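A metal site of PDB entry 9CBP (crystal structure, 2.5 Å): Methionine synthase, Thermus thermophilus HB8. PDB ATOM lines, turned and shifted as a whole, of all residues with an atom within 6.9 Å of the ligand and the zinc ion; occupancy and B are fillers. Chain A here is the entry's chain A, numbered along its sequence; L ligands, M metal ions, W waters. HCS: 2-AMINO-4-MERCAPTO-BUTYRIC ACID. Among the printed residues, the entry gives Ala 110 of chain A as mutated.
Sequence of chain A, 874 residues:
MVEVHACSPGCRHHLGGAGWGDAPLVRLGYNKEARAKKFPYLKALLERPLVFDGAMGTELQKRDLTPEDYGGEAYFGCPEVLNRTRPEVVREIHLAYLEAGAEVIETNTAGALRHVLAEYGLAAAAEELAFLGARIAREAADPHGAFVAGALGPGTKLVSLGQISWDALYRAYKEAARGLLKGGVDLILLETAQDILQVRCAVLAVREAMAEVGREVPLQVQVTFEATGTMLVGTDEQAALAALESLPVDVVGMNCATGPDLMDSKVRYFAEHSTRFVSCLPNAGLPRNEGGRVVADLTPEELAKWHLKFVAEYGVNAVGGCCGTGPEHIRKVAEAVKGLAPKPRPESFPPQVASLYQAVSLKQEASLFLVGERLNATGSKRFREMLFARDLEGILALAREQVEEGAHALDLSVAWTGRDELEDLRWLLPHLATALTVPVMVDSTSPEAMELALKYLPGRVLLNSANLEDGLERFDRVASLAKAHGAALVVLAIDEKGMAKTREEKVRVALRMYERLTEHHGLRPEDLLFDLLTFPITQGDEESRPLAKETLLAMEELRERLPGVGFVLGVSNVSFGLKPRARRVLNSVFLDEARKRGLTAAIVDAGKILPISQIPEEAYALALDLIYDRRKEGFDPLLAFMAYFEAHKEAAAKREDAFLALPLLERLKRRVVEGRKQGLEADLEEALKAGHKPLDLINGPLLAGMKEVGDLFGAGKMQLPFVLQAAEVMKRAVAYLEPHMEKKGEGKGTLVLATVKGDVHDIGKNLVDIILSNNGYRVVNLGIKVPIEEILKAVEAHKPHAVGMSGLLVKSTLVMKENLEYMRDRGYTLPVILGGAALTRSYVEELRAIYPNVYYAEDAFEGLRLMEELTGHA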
ATOM      1  N   ASP A  53     -13.256 -11.062  13.858  1.00  0.00           N
ATOM      2  CA  ASP A  53     -12.585 -12.103  13.122  1.00  0.00           C
ATOM      3  C   ASP A  53     -13.429 -12.511  11.910  1.00  0.00           C
ATOM      4  O   ASP A  53     -14.498 -11.936  11.645  1.00  0.00           O
ATOM      5  CB  ASP A  53     -12.196 -13.240  14.029  1.00  0.00           C
ATOM      6  CG  ASP A  53     -13.346 -13.922  14.739  1.00  0.00           C
ATOM      7  OD1 ASP A  53     -14.287 -13.244  15.008  1.00  0.00           O
ATOM      8  OD2 ASP A  53     -13.206 -15.108  15.050  1.00  0.00           O
ATOM      9  N   GLY A  54     -12.954 -13.572  11.241  1.00  0.00           N
ATOM     10  CA  GLY A  54     -13.546 -14.129  10.036  1.00  0.00           C
ATOM     11  C   GLY A  54     -14.080 -15.509  10.375  1.00  0.00           C
ATOM     12  O   GLY A  54     -14.326 -15.760  11.552  1.00  0.00           O
ATOM     13  N   ALA A  55     -14.120 -16.438   9.411  1.00  0.00           N
ATOM     14  CA  ALA A  55     -14.682 -17.754   9.721  1.00  0.00           C
ATOM     15  C   ALA A  55     -13.714 -18.583  10.570  1.00  0.00           C
ATOM     16  O   ALA A  55     -12.527 -18.432  10.435  1.00  0.00           O
ATOM     17  CB  ALA A  55     -15.008 -18.477   8.466  1.00  0.00           C
ATOM     18  N   MET A  56     -14.255 -19.408  11.468  1.00  0.00           N
ATOM     19  CA  MET A  56     -13.585 -20.459  12.196  1.00  0.00           C
ATOM     20  C   MET A  56     -13.736 -21.767  11.400  1.00  0.00           C
ATOM     21  O   MET A  56     -12.731 -22.345  11.044  1.00  0.00           O
ATOM     22  CB  MET A  56     -14.161 -20.583  13.613  1.00  0.00           C
ATOM     23  CG  MET A  56     -13.643 -21.774  14.434  1.00  0.00           C
ATOM     24  SD  MET A  56     -11.862 -21.847  14.727  1.00  0.00           S
ATOM     25  CE  MET A  56     -11.587 -20.345  15.677  1.00  0.00           C
ATOM     26  N   GLY A  57     -14.982 -22.188  11.102  1.00  0.00           N
ATOM     27  CA  GLY A  57     -15.311 -23.471  10.478  1.00  0.00           C
ATOM     28  C   GLY A  57     -14.546 -23.665   9.175  1.00  0.00           C
ATOM     29  O   GLY A  57     -13.886 -24.702   9.040  1.00  0.00           O
ATOM     30  N   THR A  58     -14.579 -22.654   8.248  1.00  0.00           N
ATOM     31  CA  THR A  58     -13.953 -22.801   6.937  1.00  0.00           C
ATOM     32  C   THR A  58     -12.421 -22.750   7.037  1.00  0.00           C
ATOM     33  O   THR A  58     -11.721 -23.307   6.194  1.00  0.00           O
ATOM     34  CB  THR A  58     -14.570 -21.857   5.891  1.00  0.00           C
ATOM     35  OG1 THR A  58     -14.167 -20.527   6.163  1.00  0.00           O
ATOM     36  CG2 THR A  58     -16.099 -21.951   5.799  1.00  0.00           C
ATOM     37  N   PRO A  79     -16.817 -29.296  14.985  1.00  0.00           N
ATOM     38  CA  PRO A  79     -15.816 -28.280  15.329  1.00  0.00           C
ATOM     39  C   PRO A  79     -15.517 -28.089  16.830  1.00  0.00           C
ATOM     40  O   PRO A  79     -14.368 -27.901  17.190  1.00  0.00           O
ATOM     41  CB  PRO A  79     -16.329 -26.958  14.721  1.00  0.00           C
ATOM     42  CG  PRO A  79     -17.515 -27.356  13.888  1.00  0.00           C
ATOM     43  CD  PRO A  79     -17.991 -28.715  14.335  1.00  0.00           C
ATOM     44  N   GLU A 106     -14.290 -14.632  18.049  1.00  0.00           N
ATOM     45  CA  GLU A 106     -15.406 -15.488  18.429  1.00  0.00           C
ATOM     46  C   GLU A 106     -14.913 -16.886  18.805  1.00  0.00           C
ATOM     47  O   GLU A 106     -14.078 -17.448  18.136  1.00  0.00           O
ATOM     48  CB  GLU A 106     -16.345 -15.644  17.242  1.00  0.00           C
ATOM     49  CG  GLU A 106     -16.931 -14.330  16.736  1.00  0.00           C
ATOM     50  CD  GLU A 106     -18.063 -14.528  15.745  1.00  0.00           C
ATOM     51  OE1 GLU A 106     -18.720 -15.559  15.691  1.00  0.00           O
ATOM     52  OE2 GLU A 106     -18.298 -13.535  15.070  1.00  0.00           O
ATOM     53  N   THR A 107     -15.493 -17.421  19.874  1.00  0.00           N
ATOM     54  CA  THR A 107     -15.164 -18.726  20.421  1.00  0.00           C
ATOM     55  C   THR A 107     -15.633 -19.793  19.433  1.00  0.00           C
ATOM     56  O   THR A 107     -16.641 -19.623  18.787  1.00  0.00           O
ATOM     57  CB  THR A 107     -15.822 -18.871  21.801  1.00  0.00           C
ATOM     58  OG1 THR A 107     -17.244 -18.670  21.706  1.00  0.00           O
ATOM     59  CG2 THR A 107     -15.294 -17.846  22.785  1.00  0.00           C
ATOM     60  N   ASN A 108     -14.901 -20.909  19.316  1.00  0.00           N
ATOM     61  CA  ASN A 108     -15.329 -22.032  18.487  1.00  0.00           C
ATOM     62  C   ASN A 108     -16.481 -22.807  19.214  1.00  0.00           C
ATOM     63  O   ASN A 108     -16.287 -23.925  19.669  1.00  0.00           O
ATOM     64  CB  ASN A 108     -14.067 -22.832  18.148  1.00  0.00           C
ATOM     65  CG  ASN A 108     -14.356 -24.068  17.333  1.00  0.00           C
ATOM     66  OD1 ASN A 108     -15.184 -23.998  16.408  1.00  0.00           O
ATOM     67  ND2 ASN A 108     -13.791 -25.205  17.729  1.00  0.00           N
ATOM     68  N   THR A 109     -17.672 -22.194  19.338  1.00  0.00           N
ATOM     69  CA  THR A 109     -18.748 -22.719  20.185  1.00  0.00           C
ATOM     70  C   THR A 109     -20.143 -22.587  19.535  1.00  0.00           C
ATOM     71  O   THR A 109     -21.138 -22.885  20.199  1.00  0.00           O
ATOM     72  CB  THR A 109     -18.728 -22.020  21.545  1.00  0.00           C
ATOM     73  OG1 THR A 109     -18.721 -20.627  21.275  1.00  0.00           O
ATOM     74  CG2 THR A 109     -17.511 -22.358  22.387  1.00  0.00           C
ATOM     75  N   ALA A 110     -20.243 -22.256  18.238  1.00  0.00           N
ATOM     76  CA  ALA A 110     -21.524 -21.997  17.602  1.00  0.00           C
ATOM     77  C   ALA A 110     -22.472 -23.171  17.736  1.00  0.00           C
ATOM     78  O   ALA A 110     -23.658 -22.964  17.971  1.00  0.00           O
ATOM     79  CB  ALA A 110     -21.342 -21.594  16.168  1.00  0.00           C
ATOM     80  N   ALA A 151     -19.825 -17.183  21.148  1.00  0.00           N
ATOM     81  CA  ALA A 151     -20.688 -17.365  19.992  1.00  0.00           C
ATOM     82  C   ALA A 151     -21.556 -18.594  20.218  1.00  0.00           C
ATOM     83  O   ALA A 151     -21.016 -19.677  20.452  1.00  0.00           O
ATOM     84  CB  ALA A 151     -19.871 -17.536  18.747  1.00  0.00           C
ATOM     85  N   GLY A 153     -24.910 -20.368  17.992  1.00  0.00           N
ATOM     86  CA  GLY A 153     -25.587 -20.349  16.708  1.00  0.00           C
ATOM     87  C   GLY A 153     -27.009 -20.782  16.927  1.00  0.00           C
ATOM     88  O   GLY A 153     -27.361 -21.018  18.077  1.00  0.00           O
ATOM     89  N   PRO A 154     -27.796 -21.017  15.850  1.00  0.00           N
ATOM     90  CA  PRO A 154     -29.239 -21.329  15.936  1.00  0.00           C
ATOM     91  C   PRO A 154     -29.632 -22.775  16.222  1.00  0.00           C
ATOM     92  O   PRO A 154     -30.816 -23.086  16.451  1.00  0.00           O
ATOM     93  CB  PRO A 154     -29.708 -21.048  14.484  1.00  0.00           C
ATOM     94  CG  PRO A 154     -28.464 -21.479  13.660  1.00  0.00           C
ATOM     95  CD  PRO A 154     -27.318 -20.938  14.448  1.00  0.00           C
ATOM     96  N   LEU A 189     -22.661 -13.636  22.056  1.00  0.00           N
ATOM     97  CA  LEU A 189     -23.009 -13.353  20.688  1.00  0.00           C
ATOM     98  C   LEU A 189     -23.954 -14.440  20.235  1.00  0.00           C
ATOM     99  O   LEU A 189     -23.526 -15.576  20.106  1.00  0.00           O
ATOM    100  CB  LEU A 189     -21.767 -13.321  19.811  1.00  0.00           C
ATOM    101  CG  LEU A 189     -21.998 -13.331  18.305  1.00  0.00           C
ATOM    102  CD1 LEU A 189     -22.886 -12.232  17.767  1.00  0.00           C
ATOM    103  CD2 LEU A 189     -20.694 -13.169  17.630  1.00  0.00           C
ATOM    104  N   GLU A 191     -25.786 -15.694  17.103  1.00  0.00           N
ATOM    105  CA  GLU A 191     -25.443 -15.437  15.695  1.00  0.00           C
ATOM    106  C   GLU A 191     -26.105 -16.434  14.736  1.00  0.00           C
ATOM    107  O   GLU A 191     -26.634 -17.473  15.171  1.00  0.00           O
ATOM    108  CB  GLU A 191     -23.958 -15.486  15.434  1.00  0.00           C
ATOM    109  CG  GLU A 191     -23.331 -16.830  15.818  1.00  0.00           C
ATOM    110  CD  GLU A 191     -21.897 -16.981  15.335  1.00  0.00           C
ATOM    111  OE1 GLU A 191     -21.302 -15.935  14.900  1.00  0.00           O
ATOM    112  OE2 GLU A 191     -21.392 -18.149  15.404  1.00  0.00           O
ATOM    113  N   THR A 192     -26.130 -16.063  13.428  1.00  0.00           N
ATOM    114  CA  THR A 192     -26.726 -16.869  12.343  1.00  0.00           C
ATOM    115  C   THR A 192     -28.159 -17.257  12.701  1.00  0.00           C
ATOM    116  O   THR A 192     -28.553 -18.389  12.497  1.00  0.00           O
ATOM    117  CB  THR A 192     -25.885 -18.134  12.080  1.00  0.00           C
ATOM    118  OG1 THR A 192     -24.509 -17.849  12.339  1.00  0.00           O
ATOM    119  CG2 THR A 192     -26.034 -18.637  10.650  1.00  0.00           C
ATOM    120  N   THR A 224     -29.593 -14.047  10.307  1.00  0.00           N
ATOM    121  CA  THR A 224     -29.171 -14.348   8.967  1.00  0.00           C
ATOM    122  C   THR A 224     -30.329 -14.085   8.007  1.00  0.00           C
ATOM    123  O   THR A 224     -31.343 -14.751   8.101  1.00  0.00           O
ATOM    124  CB  THR A 224     -28.758 -15.809   8.869  1.00  0.00           C
ATOM    125  OG1 THR A 224     -27.631 -15.927   9.717  1.00  0.00           O
ATOM    126  CG2 THR A 224     -28.113 -16.139   7.529  1.00  0.00           C
ATOM    127  N   ASN A 255     -25.178 -11.782   9.884  1.00  0.00           N
ATOM    128  CA  ASN A 255     -24.018 -12.559   9.504  1.00  0.00           C
ATOM    129  C   ASN A 255     -24.536 -13.657   8.602  1.00  0.00           C
ATOM    130  O   ASN A 255     -25.670 -14.101   8.759  1.00  0.00           O
ATOM    131  CB  ASN A 255     -23.177 -13.045  10.733  1.00  0.00           C
ATOM    132  CG  ASN A 255     -23.856 -14.128  11.559  1.00  0.00           C
ATOM    133  OD1 ASN A 255     -24.821 -13.875  12.344  1.00  0.00           O
ATOM    134  ND2 ASN A 255     -23.449 -15.373  11.317  1.00  0.00           N
ATOM    135  N   CYS A 256     -23.698 -14.061   7.656  1.00  0.00           N
ATOM    136  CA  CYS A 256     -23.806 -15.322   6.938  1.00  0.00           C
ATOM    137  C   CYS A 256     -24.814 -15.207   5.802  1.00  0.00           C
ATOM    138  O   CYS A 256     -25.347 -14.091   5.557  1.00  0.00           O
ATOM    139  CB  CYS A 256     -24.114 -16.554   7.796  1.00  0.00           C
ATOM    140  SG  CYS A 256     -23.351 -18.082   7.149  1.00  0.00           S
ATOM    141  N   ALA A 257     -24.946 -16.376   5.116  1.00  0.00           N
ATOM    142  CA  ALA A 257     -25.841 -16.623   3.988  1.00  0.00           C
ATOM    143  C   ALA A 257     -25.459 -15.962   2.663  1.00  0.00           C
ATOM    144  O   ALA A 257     -25.601 -16.599   1.622  1.00  0.00           O
ATOM    145  CB  ALA A 257     -27.271 -16.297   4.290  1.00  0.00           C
ATOM    146  N   LEU A 281     -21.379  -9.118   9.368  1.00  0.00           N
ATOM    147  CA  LEU A 281     -20.337 -10.096   9.051  1.00  0.00           C
ATOM    148  C   LEU A 281     -20.756 -10.923   7.838  1.00  0.00           C
ATOM    149  O   LEU A 281     -21.217 -12.041   7.986  1.00  0.00           O
ATOM    150  CB  LEU A 281     -19.869 -11.020  10.189  1.00  0.00           C
ATOM    151  CG  LEU A 281     -19.401 -10.316  11.477  1.00  0.00           C
ATOM    152  CD1 LEU A 281     -20.531  -9.918  12.375  1.00  0.00           C
ATOM    153  CD2 LEU A 281     -18.520 -11.236  12.201  1.00  0.00           C
ATOM    154  N   ASN A 283     -20.506 -13.371   4.483  1.00  0.00           N
ATOM    155  CA  ASN A 283     -19.928 -14.635   4.064  1.00  0.00           C
ATOM    156  C   ASN A 283     -19.216 -14.333   2.731  1.00  0.00           C
ATOM    157  O   ASN A 283     -19.393 -13.222   2.169  1.00  0.00           O
ATOM    158  CB  ASN A 283     -21.065 -15.681   4.109  1.00  0.00           C
ATOM    159  CG  ASN A 283     -21.296 -16.637   2.926  1.00  0.00           C
ATOM    160  OD1 ASN A 283     -21.419 -16.306   1.736  1.00  0.00           O
ATOM    161  ND2 ASN A 283     -21.463 -17.894   3.234  1.00  0.00           N
ATOM    162  N   GLY A 321     -16.179 -11.020   9.164  1.00  0.00           N
ATOM    163  CA  GLY A 321     -16.628 -11.945   8.133  1.00  0.00           C
ATOM    164  C   GLY A 321     -17.150 -13.255   8.691  1.00  0.00           C
ATOM    165  O   GLY A 321     -16.752 -13.626   9.803  1.00  0.00           O
ATOM    166  N   CYS A 322     -17.967 -13.950   7.886  1.00  0.00           N
ATOM    167  CA  CYS A 322     -18.447 -15.283   8.249  1.00  0.00           C
ATOM    168  C   CYS A 322     -17.790 -16.320   7.342  1.00  0.00           C
ATOM    169  O   CYS A 322     -16.756 -16.054   6.767  1.00  0.00           O
ATOM    170  CB  CYS A 322     -19.977 -15.320   8.202  1.00  0.00           C
ATOM    171  SG  CYS A 322     -20.666 -16.510   9.351  1.00  0.00           S
ATOM    172  N   CYS A 323     -18.436 -17.489   7.201  1.00  0.00           N
ATOM    173  CA  CYS A 323     -18.061 -18.578   6.317  1.00  0.00           C
ATOM    174  C   CYS A 323     -17.470 -18.111   4.966  1.00  0.00           C
ATOM    175  O   CYS A 323     -18.110 -17.345   4.258  1.00  0.00           O
ATOM    176  CB  CYS A 323     -19.233 -19.525   6.106  1.00  0.00           C
ATOM    177  SG  CYS A 323     -19.911 -20.173   7.641  1.00  0.00           S
ATOM    178  N   GLY A 324     -16.256 -18.593   4.666  1.00  0.00           N
ATOM    179  CA  GLY A 324     -15.518 -18.335   3.445  1.00  0.00           C
ATOM    180  C   GLY A 324     -14.548 -17.167   3.568  1.00  0.00           C
ATOM    181  O   GLY A 324     -13.907 -16.874   2.584  1.00  0.00           O
HETATM  182  N   HCS L   1     -18.890 -18.344  14.216  1.00  0.00           N
HETATM  183  CA  HCS L   1     -19.118 -19.431  13.196  1.00  0.00           C
HETATM  184  CB  HCS L   1     -20.400 -19.099  12.389  1.00  0.00           C
HETATM  185  CG  HCS L   1     -21.279 -20.261  11.927  1.00  0.00           C
HETATM  186  SD  HCS L   1     -22.270 -19.978  10.432  1.00  0.00           S
HETATM  187  C   HCS L   1     -17.837 -19.706  12.342  1.00  0.00           C
HETATM  188  OXT HCS L   1     -17.604 -20.896  11.933  1.00  0.00           O
HETATM  189  O   HCS L   1     -17.116 -18.725  11.836  1.00  0.00           O
HETATM  190 ZN    ZN M   1     -21.539 -18.590   8.652  1.00  0.00          ZN
HETATM  191  O   HOH W   1     -17.315 -20.024  16.381  1.00  0.00           O
HETATM  192  O   HOH W   2     -17.060 -21.096   9.349  1.00  0.00           O
HETATM  193  O   HOH W   3     -16.080 -16.683  13.800  1.00  0.00           O
HETATM  194  O   HOH W   4     -18.962 -15.701  11.924  1.00  0.00           O
HETATM  195  O   HOH W   5     -23.416 -19.877  13.990  1.00  0.00           O
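N of Met 56 is in hydrogen-bond range of O of the ligand.
The backbone NH of Gly 57 is in hydrogen-bond range of an oxygen (OXT) of the ligand, 3.0 Å away.
The side-chain hydroxyl (OG1) of Thr 192 lies close to a sulfur (SD) of the ligand (3.6 Å).
A nitrogen (N) of the ligand lies within salt-bridge range of the side-chain carboxylate of Glu 106 (3.2 Å).
The side-chain carboxylate (OE2) of Glu 191 is in salt-bridge range of a nitrogen (N) of the ligand, 2.8 Å away.
N of Glu 106 lies within hydrogen-bond range of OD2 of Asp 53 (3.2 Å).
N of Cys 256 sits at hydrogen-bond distance from O of Leu 281, at 3.2 Å.
N of Thr 192 lies within hydrogen-bond range of OD1 of Asn 255, 2.8 Å away.
SG of Cys 322 sits close to ND2 of Asn 255 (3.6 Å).
OE1 of Glu 191 sits close to OE1 of Glu 106, 2.7 Å away.
Ala 55 touches the ligand.
Hydrophobic or aromatic side chains that line the ligand: Ala 55 and Met 56.
Along chain A the residues within 4 Å of the ligand span positions 55 to 323.
Of the 28 residues printed, 3 come within 4 Å of the zinc ion.
Along chain A the residues within 4 Å of the zinc ion span positions 256 to 323.
The nearest printed residue that does not touch the zinc ion is Asn 255 (4.6 Å).
The zinc ion is bound by the side-chain sulfur (SG) of Cys 322 (2.4 Å), a sulfur (SD) of the ligand (2.4 Å), the side-chain sulfur (SG) of Cys 256 (2.4 Å) and the side-chain sulfur (SG) of Cys 323 (2.5 Å).
Water W2 lies within hydrogen-bond range of an oxygen (OXT) of the ligand, the backbone NH (N) of Gly 57 and the backbone NH (N) of Thr 58.
Water W5 lies within hydrogen-bond range of the side-chain hydroxyl (OG1) of Thr 192 (2.8 Å) and the side-chain carboxylate (OE2) of Glu 191 (3.0 Å).
Water W3 lies within hydrogen-bond range of the backbone carbonyl oxygen of Gly 54, an oxygen (O) of the ligand and the side-chain carboxylate of Glu 106.
Water W1 bridges O of Thr 107 (2.5 Å) and N of the ligand (3.2 Å).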
